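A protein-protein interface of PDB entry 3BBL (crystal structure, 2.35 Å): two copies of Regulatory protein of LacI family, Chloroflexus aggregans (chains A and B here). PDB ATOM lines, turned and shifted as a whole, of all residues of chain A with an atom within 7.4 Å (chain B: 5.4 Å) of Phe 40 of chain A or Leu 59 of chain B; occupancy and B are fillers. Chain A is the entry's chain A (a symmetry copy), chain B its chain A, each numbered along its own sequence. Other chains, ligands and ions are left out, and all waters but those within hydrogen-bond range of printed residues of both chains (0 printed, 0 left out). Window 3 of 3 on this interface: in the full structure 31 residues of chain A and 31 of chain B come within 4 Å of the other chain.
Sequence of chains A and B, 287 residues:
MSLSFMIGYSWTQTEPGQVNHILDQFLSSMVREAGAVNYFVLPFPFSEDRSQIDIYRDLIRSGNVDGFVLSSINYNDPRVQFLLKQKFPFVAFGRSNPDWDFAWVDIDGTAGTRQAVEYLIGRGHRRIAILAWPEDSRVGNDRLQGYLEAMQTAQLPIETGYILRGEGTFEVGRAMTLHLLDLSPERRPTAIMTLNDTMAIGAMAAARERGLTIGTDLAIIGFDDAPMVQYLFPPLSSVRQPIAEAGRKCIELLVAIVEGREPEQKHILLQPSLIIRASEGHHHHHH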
ATOM      1  N   SER A   4     -33.441  34.745  10.285  1.00  0.00           N
ATOM      2  CA  SER A   4     -32.914  33.410  10.053  1.00  0.00           C
ATOM      3  C   SER A   4     -31.698  33.510   9.137  1.00  0.00           C
ATOM      4  O   SER A   4     -30.936  32.557   8.999  1.00  0.00           O
ATOM      5  CB  SER A   4     -33.969  32.531   9.388  1.00  0.00           C
ATOM      6  OG  SER A   4     -34.284  33.029   8.098  1.00  0.00           O
ATOM      7  N   PHE A   5     -31.529  34.671   8.513  1.00  0.00           N
ATOM      8  CA  PHE A   5     -30.422  34.905   7.592  1.00  0.00           C
ATOM      9  C   PHE A   5     -30.447  33.935   6.412  1.00  0.00           C
ATOM     10  O   PHE A   5     -29.409  33.505   5.913  1.00  0.00           O
ATOM     11  CB  PHE A   5     -29.091  34.811   8.342  1.00  0.00           C
ATOM     12  CG  PHE A   5     -28.826  35.983   9.239  1.00  0.00           C
ATOM     13  CD1 PHE A   5     -28.561  37.241   8.702  1.00  0.00           C
ATOM     14  CD2 PHE A   5     -28.878  35.844  10.623  1.00  0.00           C
ATOM     15  CE1 PHE A   5     -28.351  38.350   9.533  1.00  0.00           C
ATOM     16  CE2 PHE A   5     -28.671  36.946  11.464  1.00  0.00           C
ATOM     17  CZ  PHE A   5     -28.409  38.198  10.919  1.00  0.00           C
ATOM     18  N   MET A   6     -31.651  33.593   5.971  1.00  0.00           N
ATOM     19  CA  MET A   6     -31.811  32.696   4.844  1.00  0.00           C
ATOM     20  C   MET A   6     -32.875  33.177   3.866  1.00  0.00           C
ATOM     21  O   MET A   6     -33.963  33.605   4.262  1.00  0.00           O
ATOM     22  CB  MET A   6     -32.111  31.292   5.345  1.00  0.00           C
ATOM     23  CG  MET A   6     -30.874  30.693   5.943  1.00  0.00           C
ATOM     24  SD  MET A   6     -31.129  28.855   6.445  1.00  0.00           S
ATOM     25  CE  MET A   6     -30.949  28.106   4.707  1.00  0.00           C
ATOM     26  N   ILE A   7     -32.533  33.131   2.582  1.00  0.00           N
ATOM     27  CA  ILE A   7     -33.434  33.564   1.520  1.00  0.00           C
ATOM     28  C   ILE A   7     -33.856  32.348   0.711  1.00  0.00           C
ATOM     29  O   ILE A   7     -33.019  31.619   0.180  1.00  0.00           O
ATOM     30  CB  ILE A   7     -32.732  34.590   0.598  1.00  0.00           C
ATOM     31  CG1 ILE A   7     -32.359  35.833   1.411  1.00  0.00           C
ATOM     32  CG2 ILE A   7     -33.638  34.965  -0.571  1.00  0.00           C
ATOM     33  CD1 ILE A   7     -31.278  36.684   0.788  1.00  0.00           C
ATOM     34  N   GLY A   8     -35.160  32.123   0.638  1.00  0.00           N
ATOM     35  CA  GLY A   8     -35.660  30.984  -0.107  1.00  0.00           C
ATOM     36  C   GLY A   8     -35.713  31.238  -1.599  1.00  0.00           C
ATOM     37  O   GLY A   8     -36.105  32.320  -2.047  1.00  0.00           O
ATOM     38  N   MET A  30     -26.115  34.880  -6.488  1.00  0.00           N
ATOM     39  CA  MET A  30     -26.867  35.139  -5.265  1.00  0.00           C
ATOM     40  C   MET A  30     -26.158  34.539  -4.052  1.00  0.00           C
ATOM     41  O   MET A  30     -26.019  35.193  -3.019  1.00  0.00           O
ATOM     42  CB  MET A  30     -28.301  34.597  -5.363  1.00  0.00           C
ATOM     43  CG  MET A  30     -29.139  35.392  -6.323  1.00  0.00           C
ATOM     44  SD  MET A  30     -31.097  35.227  -6.035  1.00  0.00           S
ATOM     45  CE  MET A  30     -31.214  33.323  -6.372  1.00  0.00           C
ATOM     46  N   VAL A  31     -25.690  33.301  -4.187  1.00  0.00           N
ATOM     47  CA  VAL A  31     -25.004  32.635  -3.094  1.00  0.00           C
ATOM     48  C   VAL A  31     -23.791  33.414  -2.611  1.00  0.00           C
ATOM     49  O   VAL A  31     -23.572  33.542  -1.412  1.00  0.00           O
ATOM     50  CB  VAL A  31     -24.565  31.220  -3.499  1.00  0.00           C
ATOM     51  CG1 VAL A  31     -23.631  30.633  -2.440  1.00  0.00           C
ATOM     52  CG2 VAL A  31     -25.789  30.335  -3.666  1.00  0.00           C
ATOM     53  N   ALA A  34     -25.094  36.874  -1.043  1.00  0.00           N
ATOM     54  CA  ALA A  34     -25.725  36.646   0.245  1.00  0.00           C
ATOM     55  C   ALA A  34     -24.623  36.377   1.263  1.00  0.00           C
ATOM     56  O   ALA A  34     -24.574  37.003   2.322  1.00  0.00           O
ATOM     57  CB  ALA A  34     -26.667  35.452   0.157  1.00  0.00           C
ATOM     58  N   GLY A  35     -23.734  35.452   0.922  1.00  0.00           N
ATOM     59  CA  GLY A  35     -22.635  35.107   1.804  1.00  0.00           C
ATOM     60  C   GLY A  35     -21.848  36.311   2.295  1.00  0.00           C
ATOM     61  O   GLY A  35     -21.470  36.383   3.464  1.00  0.00           O
ATOM     62  N   VAL A  37     -22.844  39.186   2.961  1.00  0.00           N
ATOM     63  CA  VAL A  37     -23.574  39.894   4.007  1.00  0.00           C
ATOM     64  C   VAL A  37     -24.158  38.899   5.006  1.00  0.00           C
ATOM     65  O   VAL A  37     -25.179  39.165   5.643  1.00  0.00           O
ATOM     66  CB  VAL A  37     -24.713  40.768   3.423  1.00  0.00           C
ATOM     67  CG1 VAL A  37     -24.126  41.892   2.591  1.00  0.00           C
ATOM     68  CG2 VAL A  37     -25.659  39.910   2.589  1.00  0.00           C
ATOM     69  N   ASN A  38     -23.503  37.747   5.122  1.00  0.00           N
ATOM     70  CA  ASN A  38     -23.899  36.692   6.048  1.00  0.00           C
ATOM     71  C   ASN A  38     -25.258  36.026   5.852  1.00  0.00           C
ATOM     72  O   ASN A  38     -25.880  35.576   6.816  1.00  0.00           O
ATOM     73  CB  ASN A  38     -23.795  37.203   7.483  1.00  0.00           C
ATOM     74  CG  ASN A  38     -22.380  37.565   7.863  1.00  0.00           C
ATOM     75  OD1 ASN A  38     -21.493  36.710   7.872  1.00  0.00           O
ATOM     76  ND2 ASN A  38     -22.155  38.836   8.171  1.00  0.00           N
ATOM     77  N   TYR A  39     -25.727  35.956   4.616  1.00  0.00           N
ATOM     78  CA  TYR A  39     -26.999  35.296   4.354  1.00  0.00           C
ATOM     79  C   TYR A  39     -26.749  34.034   3.528  1.00  0.00           C
ATOM     80  O   TYR A  39     -25.706  33.902   2.888  1.00  0.00           O
ATOM     81  CB  TYR A  39     -27.958  36.219   3.598  1.00  0.00           C
ATOM     82  CG  TYR A  39     -28.724  37.200   4.461  1.00  0.00           C
ATOM     83  CD1 TYR A  39     -28.122  38.360   4.942  1.00  0.00           C
ATOM     84  CD2 TYR A  39     -30.064  36.976   4.777  1.00  0.00           C
ATOM     85  CE1 TYR A  39     -28.837  39.275   5.715  1.00  0.00           C
ATOM     86  CE2 TYR A  39     -30.787  37.882   5.551  1.00  0.00           C
ATOM     87  CZ  TYR A  39     -30.170  39.030   6.016  1.00  0.00           C
ATOM     88  OH  TYR A  39     -30.880  39.928   6.781  1.00  0.00           O
ATOM     89  N   PHE A  40     -27.691  33.099   3.575  1.00  0.00           N
ATOM     90  CA  PHE A  40     -27.590  31.874   2.796  1.00  0.00           C
ATOM     91  C   PHE A  40     -28.841  31.801   1.945  1.00  0.00           C
ATOM     92  O   PHE A  40     -29.892  32.321   2.328  1.00  0.00           O
ATOM     93  CB  PHE A  40     -27.554  30.615   3.677  1.00  0.00           C
ATOM     94  CG  PHE A  40     -26.280  30.433   4.454  1.00  0.00           C
ATOM     95  CD1 PHE A  40     -26.096  31.070   5.675  1.00  0.00           C
ATOM     96  CD2 PHE A  40     -25.273  29.606   3.973  1.00  0.00           C
ATOM     97  CE1 PHE A  40     -24.929  30.885   6.408  1.00  0.00           C
ATOM     98  CE2 PHE A  40     -24.101  29.414   4.697  1.00  0.00           C
ATOM     99  CZ  PHE A  40     -23.929  30.054   5.919  1.00  0.00           C
ATOM    100  N   VAL A  41     -28.723  31.170   0.781  1.00  0.00           N
ATOM    101  CA  VAL A  41     -29.864  30.988  -0.096  1.00  0.00           C
ATOM    102  C   VAL A  41     -30.341  29.575   0.194  1.00  0.00           C
ATOM    103  O   VAL A  41     -29.551  28.638   0.213  1.00  0.00           O
ATOM    104  CB  VAL A  41     -29.479  31.087  -1.586  1.00  0.00           C
ATOM    105  CG1 VAL A  41     -30.690  30.757  -2.455  1.00  0.00           C
ATOM    106  CG2 VAL A  41     -28.958  32.488  -1.900  1.00  0.00           C
ATOM    107  N   LEU A  42     -31.634  29.425   0.441  1.00  0.00           N
ATOM    108  CA  LEU A  42     -32.179  28.118   0.725  1.00  0.00           C
ATOM    109  C   LEU A  42     -33.071  27.635  -0.407  1.00  0.00           C
ATOM    110  O   LEU A  42     -34.202  28.097  -0.561  1.00  0.00           O
ATOM    111  CB  LEU A  42     -32.980  28.157   2.020  1.00  0.00           C
ATOM    112  CG  LEU A  42     -33.578  26.821   2.456  1.00  0.00           C
ATOM    113  CD1 LEU A  42     -32.459  25.855   2.805  1.00  0.00           C
ATOM    114  CD2 LEU A  42     -34.504  27.029   3.645  1.00  0.00           C
ATOM    115  N   PRO A  43     -32.566  26.703  -1.227  1.00  0.00           N
ATOM    116  CA  PRO A  43     -33.349  26.167  -2.341  1.00  0.00           C
ATOM    117  C   PRO A  43     -34.439  25.241  -1.822  1.00  0.00           C
ATOM    118  O   PRO A  43     -34.234  24.516  -0.856  1.00  0.00           O
ATOM    119  CB  PRO A  43     -32.318  25.388  -3.152  1.00  0.00           C
ATOM    120  CG  PRO A  43     -31.026  26.038  -2.796  1.00  0.00           C
ATOM    121  CD  PRO A  43     -31.163  26.274  -1.324  1.00  0.00           C
ATOM    122  N   ASN A  64     -37.902  29.452   8.755  1.00  0.00           N
ATOM    123  CA  ASN A  64     -36.649  29.072   8.115  1.00  0.00           C
ATOM    124  C   ASN A  64     -36.066  30.101   7.138  1.00  0.00           C
ATOM    125  O   ASN A  64     -34.895  30.011   6.774  1.00  0.00           O
ATOM    126  CB  ASN A  64     -36.811  27.723   7.401  1.00  0.00           C
ATOM    127  CG  ASN A  64     -36.975  26.556   8.375  1.00  0.00           C
ATOM    128  OD1 ASN A  64     -36.933  26.738   9.596  1.00  0.00           O
ATOM    129  ND2 ASN A  64     -37.159  25.352   7.833  1.00  0.00           N
ATOM    130  N   VAL A  65     -36.873  31.071   6.712  1.00  0.00           N
ATOM    131  CA  VAL A  65     -36.403  32.101   5.791  1.00  0.00           C
ATOM    132  C   VAL A  65     -36.999  33.451   6.137  1.00  0.00           C
ATOM    133  O   VAL A  65     -38.074  33.526   6.713  1.00  0.00           O
ATOM    134  CB  VAL A  65     -36.781  31.778   4.329  1.00  0.00           C
ATOM    135  CG1 VAL A  65     -36.176  30.452   3.916  1.00  0.00           C
ATOM    136  CG2 VAL A  65     -38.289  31.744   4.177  1.00  0.00           C
ATOM    137  N   GLY A  67     -37.155  35.826   3.664  1.00  0.00           N
ATOM    138  CA  GLY A  67     -37.667  36.342   2.406  1.00  0.00           C
ATOM    139  C   GLY A  67     -37.468  35.374   1.253  1.00  0.00           C
ATOM    140  O   GLY A  67     -36.789  34.349   1.385  1.00  0.00           O
ATOM    141  N   ILE A 251     -30.669  39.857  -4.253  1.00  0.00           N
ATOM    142  CA  ILE A 251     -30.251  39.637  -2.875  1.00  0.00           C
ATOM    143  C   ILE A 251     -30.113  40.971  -2.148  1.00  0.00           C
ATOM    144  O   ILE A 251     -30.625  41.163  -1.051  1.00  0.00           O
ATOM    145  CB  ILE A 251     -28.899  38.893  -2.826  1.00  0.00           C
ATOM    146  CG1 ILE A 251     -29.074  37.461  -3.338  1.00  0.00           C
ATOM    147  CG2 ILE A 251     -28.345  38.893  -1.407  1.00  0.00           C
ATOM    148  CD1 ILE A 251     -30.005  36.608  -2.493  1.00  0.00           C
ATOM    149  N   LEU B  42     -28.129  23.324   1.524  1.00  0.00           N
ATOM    150  CA  LEU B  42     -27.702  24.668   1.835  1.00  0.00           C
ATOM    151  C   LEU B  42     -26.434  25.033   1.080  1.00  0.00           C
ATOM    152  O   LEU B  42     -25.342  24.582   1.427  1.00  0.00           O
ATOM    153  CB  LEU B  42     -27.458  24.805   3.333  1.00  0.00           C
ATOM    154  CG  LEU B  42     -27.041  26.199   3.799  1.00  0.00           C
ATOM    155  CD1 LEU B  42     -28.185  27.172   3.575  1.00  0.00           C
ATOM    156  CD2 LEU B  42     -26.644  26.156   5.268  1.00  0.00           C
ATOM    157  N   PRO B  43     -26.564  25.846   0.024  1.00  0.00           N
ATOM    158  CA  PRO B  43     -25.403  26.264  -0.762  1.00  0.00           C
ATOM    159  C   PRO B  43     -24.571  27.271   0.019  1.00  0.00           C
ATOM    160  O   PRO B  43     -25.113  28.102   0.738  1.00  0.00           O
ATOM    161  CB  PRO B  43     -26.027  26.914  -1.993  1.00  0.00           C
ATOM    162  CG  PRO B  43     -27.371  26.280  -2.082  1.00  0.00           C
ATOM    163  CD  PRO B  43     -27.814  26.227  -0.652  1.00  0.00           C
ATOM    164  N   PHE B  44     -23.258  27.181  -0.115  1.00  0.00           N
ATOM    165  CA  PHE B  44     -22.360  28.118   0.537  1.00  0.00           C
ATOM    166  C   PHE B  44     -21.270  28.436  -0.482  1.00  0.00           C
ATOM    167  O   PHE B  44     -20.991  27.633  -1.368  1.00  0.00           O
ATOM    168  CB  PHE B  44     -21.783  27.527   1.841  1.00  0.00           C
ATOM    169  CG  PHE B  44     -20.983  26.275   1.661  1.00  0.00           C
ATOM    170  CD1 PHE B  44     -19.627  26.335   1.372  1.00  0.00           C
ATOM    171  CD2 PHE B  44     -21.580  25.028   1.823  1.00  0.00           C
ATOM    172  CE1 PHE B  44     -18.866  25.168   1.251  1.00  0.00           C
ATOM    173  CE2 PHE B  44     -20.833  23.852   1.703  1.00  0.00           C
ATOM    174  CZ  PHE B  44     -19.471  23.924   1.418  1.00  0.00           C
ATOM    175  N   PRO B  45     -20.659  29.627  -0.386  1.00  0.00           N
ATOM    176  CA  PRO B  45     -19.606  30.028  -1.320  1.00  0.00           C
ATOM    177  C   PRO B  45     -18.469  29.023  -1.416  1.00  0.00           C
ATOM    178  O   PRO B  45     -17.971  28.528  -0.408  1.00  0.00           O
ATOM    179  CB  PRO B  45     -19.157  31.376  -0.767  1.00  0.00           C
ATOM    180  CG  PRO B  45     -20.433  31.922  -0.197  1.00  0.00           C
ATOM    181  CD  PRO B  45     -20.968  30.721   0.550  1.00  0.00           C
ATOM    182  N   ASP B  54     -11.987  26.967   5.992  1.00  0.00           N
ATOM    183  CA  ASP B  54     -12.623  27.767   7.029  1.00  0.00           C
ATOM    184  C   ASP B  54     -14.138  27.662   7.027  1.00  0.00           C
ATOM    185  O   ASP B  54     -14.751  27.394   8.060  1.00  0.00           O
ATOM    186  CB  ASP B  54     -12.213  29.228   6.882  1.00  0.00           C
ATOM    187  CG  ASP B  54     -10.976  29.562   7.682  1.00  0.00           C
ATOM    188  OD1 ASP B  54     -10.182  28.637   7.964  1.00  0.00           O
ATOM    189  OD2 ASP B  54     -10.796  30.751   8.022  1.00  0.00           O
ATOM    190  N   ILE B  55     -14.736  27.872   5.859  1.00  0.00           N
ATOM    191  CA  ILE B  55     -16.180  27.811   5.714  1.00  0.00           C
ATOM    192  C   ILE B  55     -16.749  26.471   6.194  1.00  0.00           C
ATOM    193  O   ILE B  55     -17.840  26.430   6.765  1.00  0.00           O
ATOM    194  CB  ILE B  55     -16.582  28.080   4.247  1.00  0.00           C
ATOM    195  CG1 ILE B  55     -18.101  27.989   4.088  1.00  0.00           C
ATOM    196  CG2 ILE B  55     -15.859  27.114   3.332  1.00  0.00           C
ATOM    197  CD1 ILE B  55     -18.875  29.042   4.857  1.00  0.00           C
ATOM    198  N   TYR B  56     -16.022  25.380   5.972  1.00  0.00           N
ATOM    199  CA  TYR B  56     -16.498  24.077   6.430  1.00  0.00           C
ATOM    200  C   TYR B  56     -16.455  24.048   7.953  1.00  0.00           C
ATOM    201  O   TYR B  56     -17.378  23.565   8.608  1.00  0.00           O
ATOM    202  CB  TYR B  56     -15.632  22.936   5.878  1.00  0.00           C
ATOM    203  CG  TYR B  56     -15.887  22.611   4.422  1.00  0.00           C
ATOM    204  CD1 TYR B  56     -15.219  23.293   3.408  1.00  0.00           C
ATOM    205  CD2 TYR B  56     -16.816  21.632   4.059  1.00  0.00           C
ATOM    206  CE1 TYR B  56     -15.467  23.013   2.072  1.00  0.00           C
ATOM    207  CE2 TYR B  56     -17.073  21.349   2.727  1.00  0.00           C
ATOM    208  CZ  TYR B  56     -16.395  22.045   1.736  1.00  0.00           C
ATOM    209  OH  TYR B  56     -16.657  21.783   0.407  1.00  0.00           O
ATOM    210  N   ARG B  57     -15.367  24.580   8.496  1.00  0.00           N
ATOM    211  CA  ARG B  57     -15.148  24.649   9.935  1.00  0.00           C
ATOM    212  C   ARG B  57     -16.290  25.440  10.588  1.00  0.00           C
ATOM    213  O   ARG B  57     -16.834  25.037  11.617  1.00  0.00           O
ATOM    214  CB  ARG B  57     -13.805  25.336  10.208  1.00  0.00           C
ATOM    215  CG  ARG B  57     -13.193  25.030  11.560  1.00  0.00           C
ATOM    216  CD  ARG B  57     -12.168  26.092  11.953  1.00  0.00           C
ATOM    217  NE  ARG B  57     -11.025  26.179  11.043  1.00  0.00           N
ATOM    218  CZ  ARG B  57     -10.089  25.242  10.918  1.00  0.00           C
ATOM    219  NH1 ARG B  57     -10.152  24.133  11.642  1.00  0.00           N
ATOM    220  NH2 ARG B  57      -9.084  25.424  10.074  1.00  0.00           N
ATOM    221  N   ASP B  58     -16.658  26.558   9.969  1.00  0.00           N
ATOM    222  CA  ASP B  58     -17.727  27.413  10.473  1.00  0.00           C
ATOM    223  C   ASP B  58     -19.090  26.736  10.450  1.00  0.00           C
ATOM    224  O   ASP B  58     -19.818  26.758  11.439  1.00  0.00           O
ATOM    225  CB  ASP B  58     -17.807  28.695   9.647  1.00  0.00           C
ATOM    226  CG  ASP B  58     -16.576  29.560   9.790  1.00  0.00           C
ATOM    227  OD1 ASP B  58     -15.459  29.005   9.826  1.00  0.00           O
ATOM    228  OD2 ASP B  58     -16.720  30.796   9.852  1.00  0.00           O
ATOM    229  N   LEU B  59     -19.438  26.135   9.316  1.00  0.00           N
ATOM    230  CA  LEU B  59     -20.736  25.486   9.178  1.00  0.00           C
ATOM    231  C   LEU B  59     -20.948  24.315  10.127  1.00  0.00           C
ATOM    232  O   LEU B  59     -22.078  24.047  10.546  1.00  0.00           O
ATOM    233  CB  LEU B  59     -20.954  25.044   7.728  1.00  0.00           C
ATOM    234  CG  LEU B  59     -21.131  26.199   6.734  1.00  0.00           C
ATOM    235  CD1 LEU B  59     -21.256  25.666   5.321  1.00  0.00           C
ATOM    236  CD2 LEU B  59     -22.356  27.008   7.113  1.00  0.00           C
ATOM    237  N   ILE B  60     -19.870  23.623  10.476  1.00  0.00           N
ATOM    238  CA  ILE B  60     -19.985  22.489  11.381  1.00  0.00           C
ATOM    239  C   ILE B  60     -20.343  22.923  12.803  1.00  0.00           C
ATOM    240  O   ILE B  60     -21.318  22.429  13.376  1.00  0.00           O
ATOM    241  CB  ILE B  60     -18.685  21.655  11.412  1.00  0.00           C
ATOM    242  CG1 ILE B  60     -18.450  21.012  10.040  1.00  0.00           C
ATOM    243  CG2 ILE B  60     -18.783  20.576  12.481  1.00  0.00           C
ATOM    244  CD1 ILE B  60     -17.158  20.233   9.929  1.00  0.00           C
ATOM    245  N   ARG B  61     -19.584  23.850  13.377  1.00  0.00           N
ATOM    246  CA  ARG B  61     -19.901  24.266  14.733  1.00  0.00           C
ATOM    247  C   ARG B  61     -21.083  25.206  14.853  1.00  0.00           C
ATOM    248  O   ARG B  61     -21.562  25.456  15.955  1.00  0.00           O
ATOM    249  CB  ARG B  61     -18.676  24.853  15.434  1.00  0.00           C
ATOM    250  CG  ARG B  61     -17.831  25.800  14.631  1.00  0.00           C
ATOM    251  CD  ARG B  61     -16.375  25.478  14.916  1.00  0.00           C
ATOM    252  NE  ARG B  61     -15.491  26.619  14.713  1.00  0.00           N
ATOM    253  CZ  ARG B  61     -14.163  26.543  14.727  1.00  0.00           C
ATOM    254  NH1 ARG B  61     -13.557  25.376  14.934  1.00  0.00           N
ATOM    255  NH2 ARG B  61     -13.441  27.638  14.538  1.00  0.00           N
ATOM    256  N   SER B  62     -21.568  25.717  13.728  1.00  0.00           N
ATOM    257  CA  SER B  62     -22.729  26.597  13.763  1.00  0.00           C
ATOM    258  C   SER B  62     -23.963  25.697  13.844  1.00  0.00           C
ATOM    259  O   SER B  62     -25.071  26.160  14.110  1.00  0.00           O
ATOM    260  CB  SER B  62     -22.809  27.456  12.498  1.00  0.00           C
ATOM    261  OG  SER B  62     -23.294  26.706  11.395  1.00  0.00           O
ATOM    262  N   GLY B  63     -23.756  24.404  13.610  1.00  0.00           N
ATOM    263  CA  GLY B  63     -24.853  23.452  13.652  1.00  0.00           C
ATOM    264  C   GLY B  63     -25.870  23.650  12.540  1.00  0.00           C
ATOM    265  O   GLY B  63     -26.957  23.079  12.578  1.00  0.00           O
ATOM    266  N   ASN B  64     -25.517  24.449  11.540  1.00  0.00           N
ATOM    267  CA  ASN B  64     -26.422  24.720  10.429  1.00  0.00           C
ATOM    268  C   ASN B  64     -26.611  23.567   9.435  1.00  0.00           C
ATOM    269  O   ASN B  64     -27.552  23.584   8.644  1.00  0.00           O
ATOM    270  CB  ASN B  64     -25.966  25.977   9.674  1.00  0.00           C
ATOM    271  CG  ASN B  64     -26.159  27.255  10.489  1.00  0.00           C
ATOM    272  OD1 ASN B  64     -26.669  27.221  11.614  1.00  0.00           O
ATOM    273  ND2 ASN B  64     -25.753  28.390   9.917  1.00  0.00           N
ATOM    274  N   VAL B  65     -25.727  22.573   9.471  1.00  0.00           N
ATOM    275  CA  VAL B  65     -25.833  21.428   8.571  1.00  0.00           C
ATOM    276  C   VAL B  65     -25.447  20.144   9.279  1.00  0.00           C
ATOM    277  O   VAL B  65     -24.676  20.165  10.227  1.00  0.00           O
ATOM    278  CB  VAL B  65     -24.916  21.581   7.338  1.00  0.00           C
ATOM    279  CG1 VAL B  65     -25.286  22.833   6.567  1.00  0.00           C
ATOM    280  CG2 VAL B  65     -23.465  21.633   7.770  1.00  0.00           C
ATOM    281  N   PHE B  68     -22.214  17.205   4.441  1.00  0.00           N
ATOM    282  CA  PHE B  68     -21.818  17.883   3.217  1.00  0.00           C
ATOM    283  C   PHE B  68     -21.752  16.941   2.028  1.00  0.00           C
ATOM    284  O   PHE B  68     -21.579  15.731   2.170  1.00  0.00           O
ATOM    285  CB  PHE B  68     -20.420  18.478   3.362  1.00  0.00           C
ATOM    286  CG  PHE B  68     -20.309  19.575   4.368  1.00  0.00           C
ATOM    287  CD1 PHE B  68     -20.718  20.865   4.056  1.00  0.00           C
ATOM    288  CD2 PHE B  68     -19.735  19.330   5.612  1.00  0.00           C
ATOM    289  CE1 PHE B  68     -20.550  21.904   4.962  1.00  0.00           C
ATOM    290  CE2 PHE B  68     -19.561  20.355   6.528  1.00  0.00           C
ATOM    291  CZ  PHE B  68     -19.968  21.649   6.205  1.00  0.00           C
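Of chain B, only Leu 42, Pro 43 and Leu 59 come within 4 Å of Phe 40 of chain A. Of chain A, only Phe 40 comes within 4 Å of Leu 59 of chain B. Printed residues of chain A within 4 Å of Leu 42 of chain B: Met 6 (3.1 Å), Phe 40 (3.5 Å) and Val 41 (3.9 Å). Of the printed residues of chain A, Pro 43 of chain B touches Val 31, Phe 40, Val 41 and Pro 43. Arg 61 of chain B touches none of the printed residues of chain A. The nearest residue of chain B that does not touch Phe 40 of chain A is Phe 44 of chain B (4.1 Å). The nearest printed residue of chain A that does not touch Leu 59 of chain B is Tyr 39 of chain A (8.8 Å).
Hydrophobic or aromatic side chains of chain A within 4 Å of the printed part of chain B: Met 6, Val 31, Phe 40 and Pro 43.
Among the printed residues, merely in contact across the chains: Val 41 of chain A with Pro 43 of chain B, Met 6 of chain A with Leu 42 of chain B, Pro 43 of chain A with Pro 43 of chain B, Phe 40 of chain A with Leu 42 of chain B, Phe 40 of chain A with Pro 43 of chain B, Phe 40 of chain A with Leu 59 of chain B, Val 31 of chain A with Pro 45 of chain B, Val 31 of chain A with Phe 44 of chain B, Val 31 of chain A with Pro 43 of chain B and Val 41 of chain A with Leu 42 of chain B.
Pro 43 of chain A touches its own counterpart, Pro 43 of chain B. Positions printed for both chains: 42, 43, 64 and 65. Of the 10 pairs that touch across the chains among the printed residues, 1 has its exchanged pair printed and touching as well.
The side-chain hydroxyl of Ser 62 of chain B sits at hydrogen-bond distance from the backbone carbonyl oxygen of Leu 59 of chain B (3.0 Å). The side-chain hydroxyl (OG) of Ser 4 of chain A sits close to the backbone NH (N) of Met 6 of chain A (3.4 Å). The backbone carbonyl oxygen (O) of Phe 5 of chain A is in hydrogen-bond range of the backbone NH (N) of Phe 40 of chain A. O of Phe 40 of chain A sits at hydrogen-bond distance from N of Ile 7 of chain A (2.8 Å).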
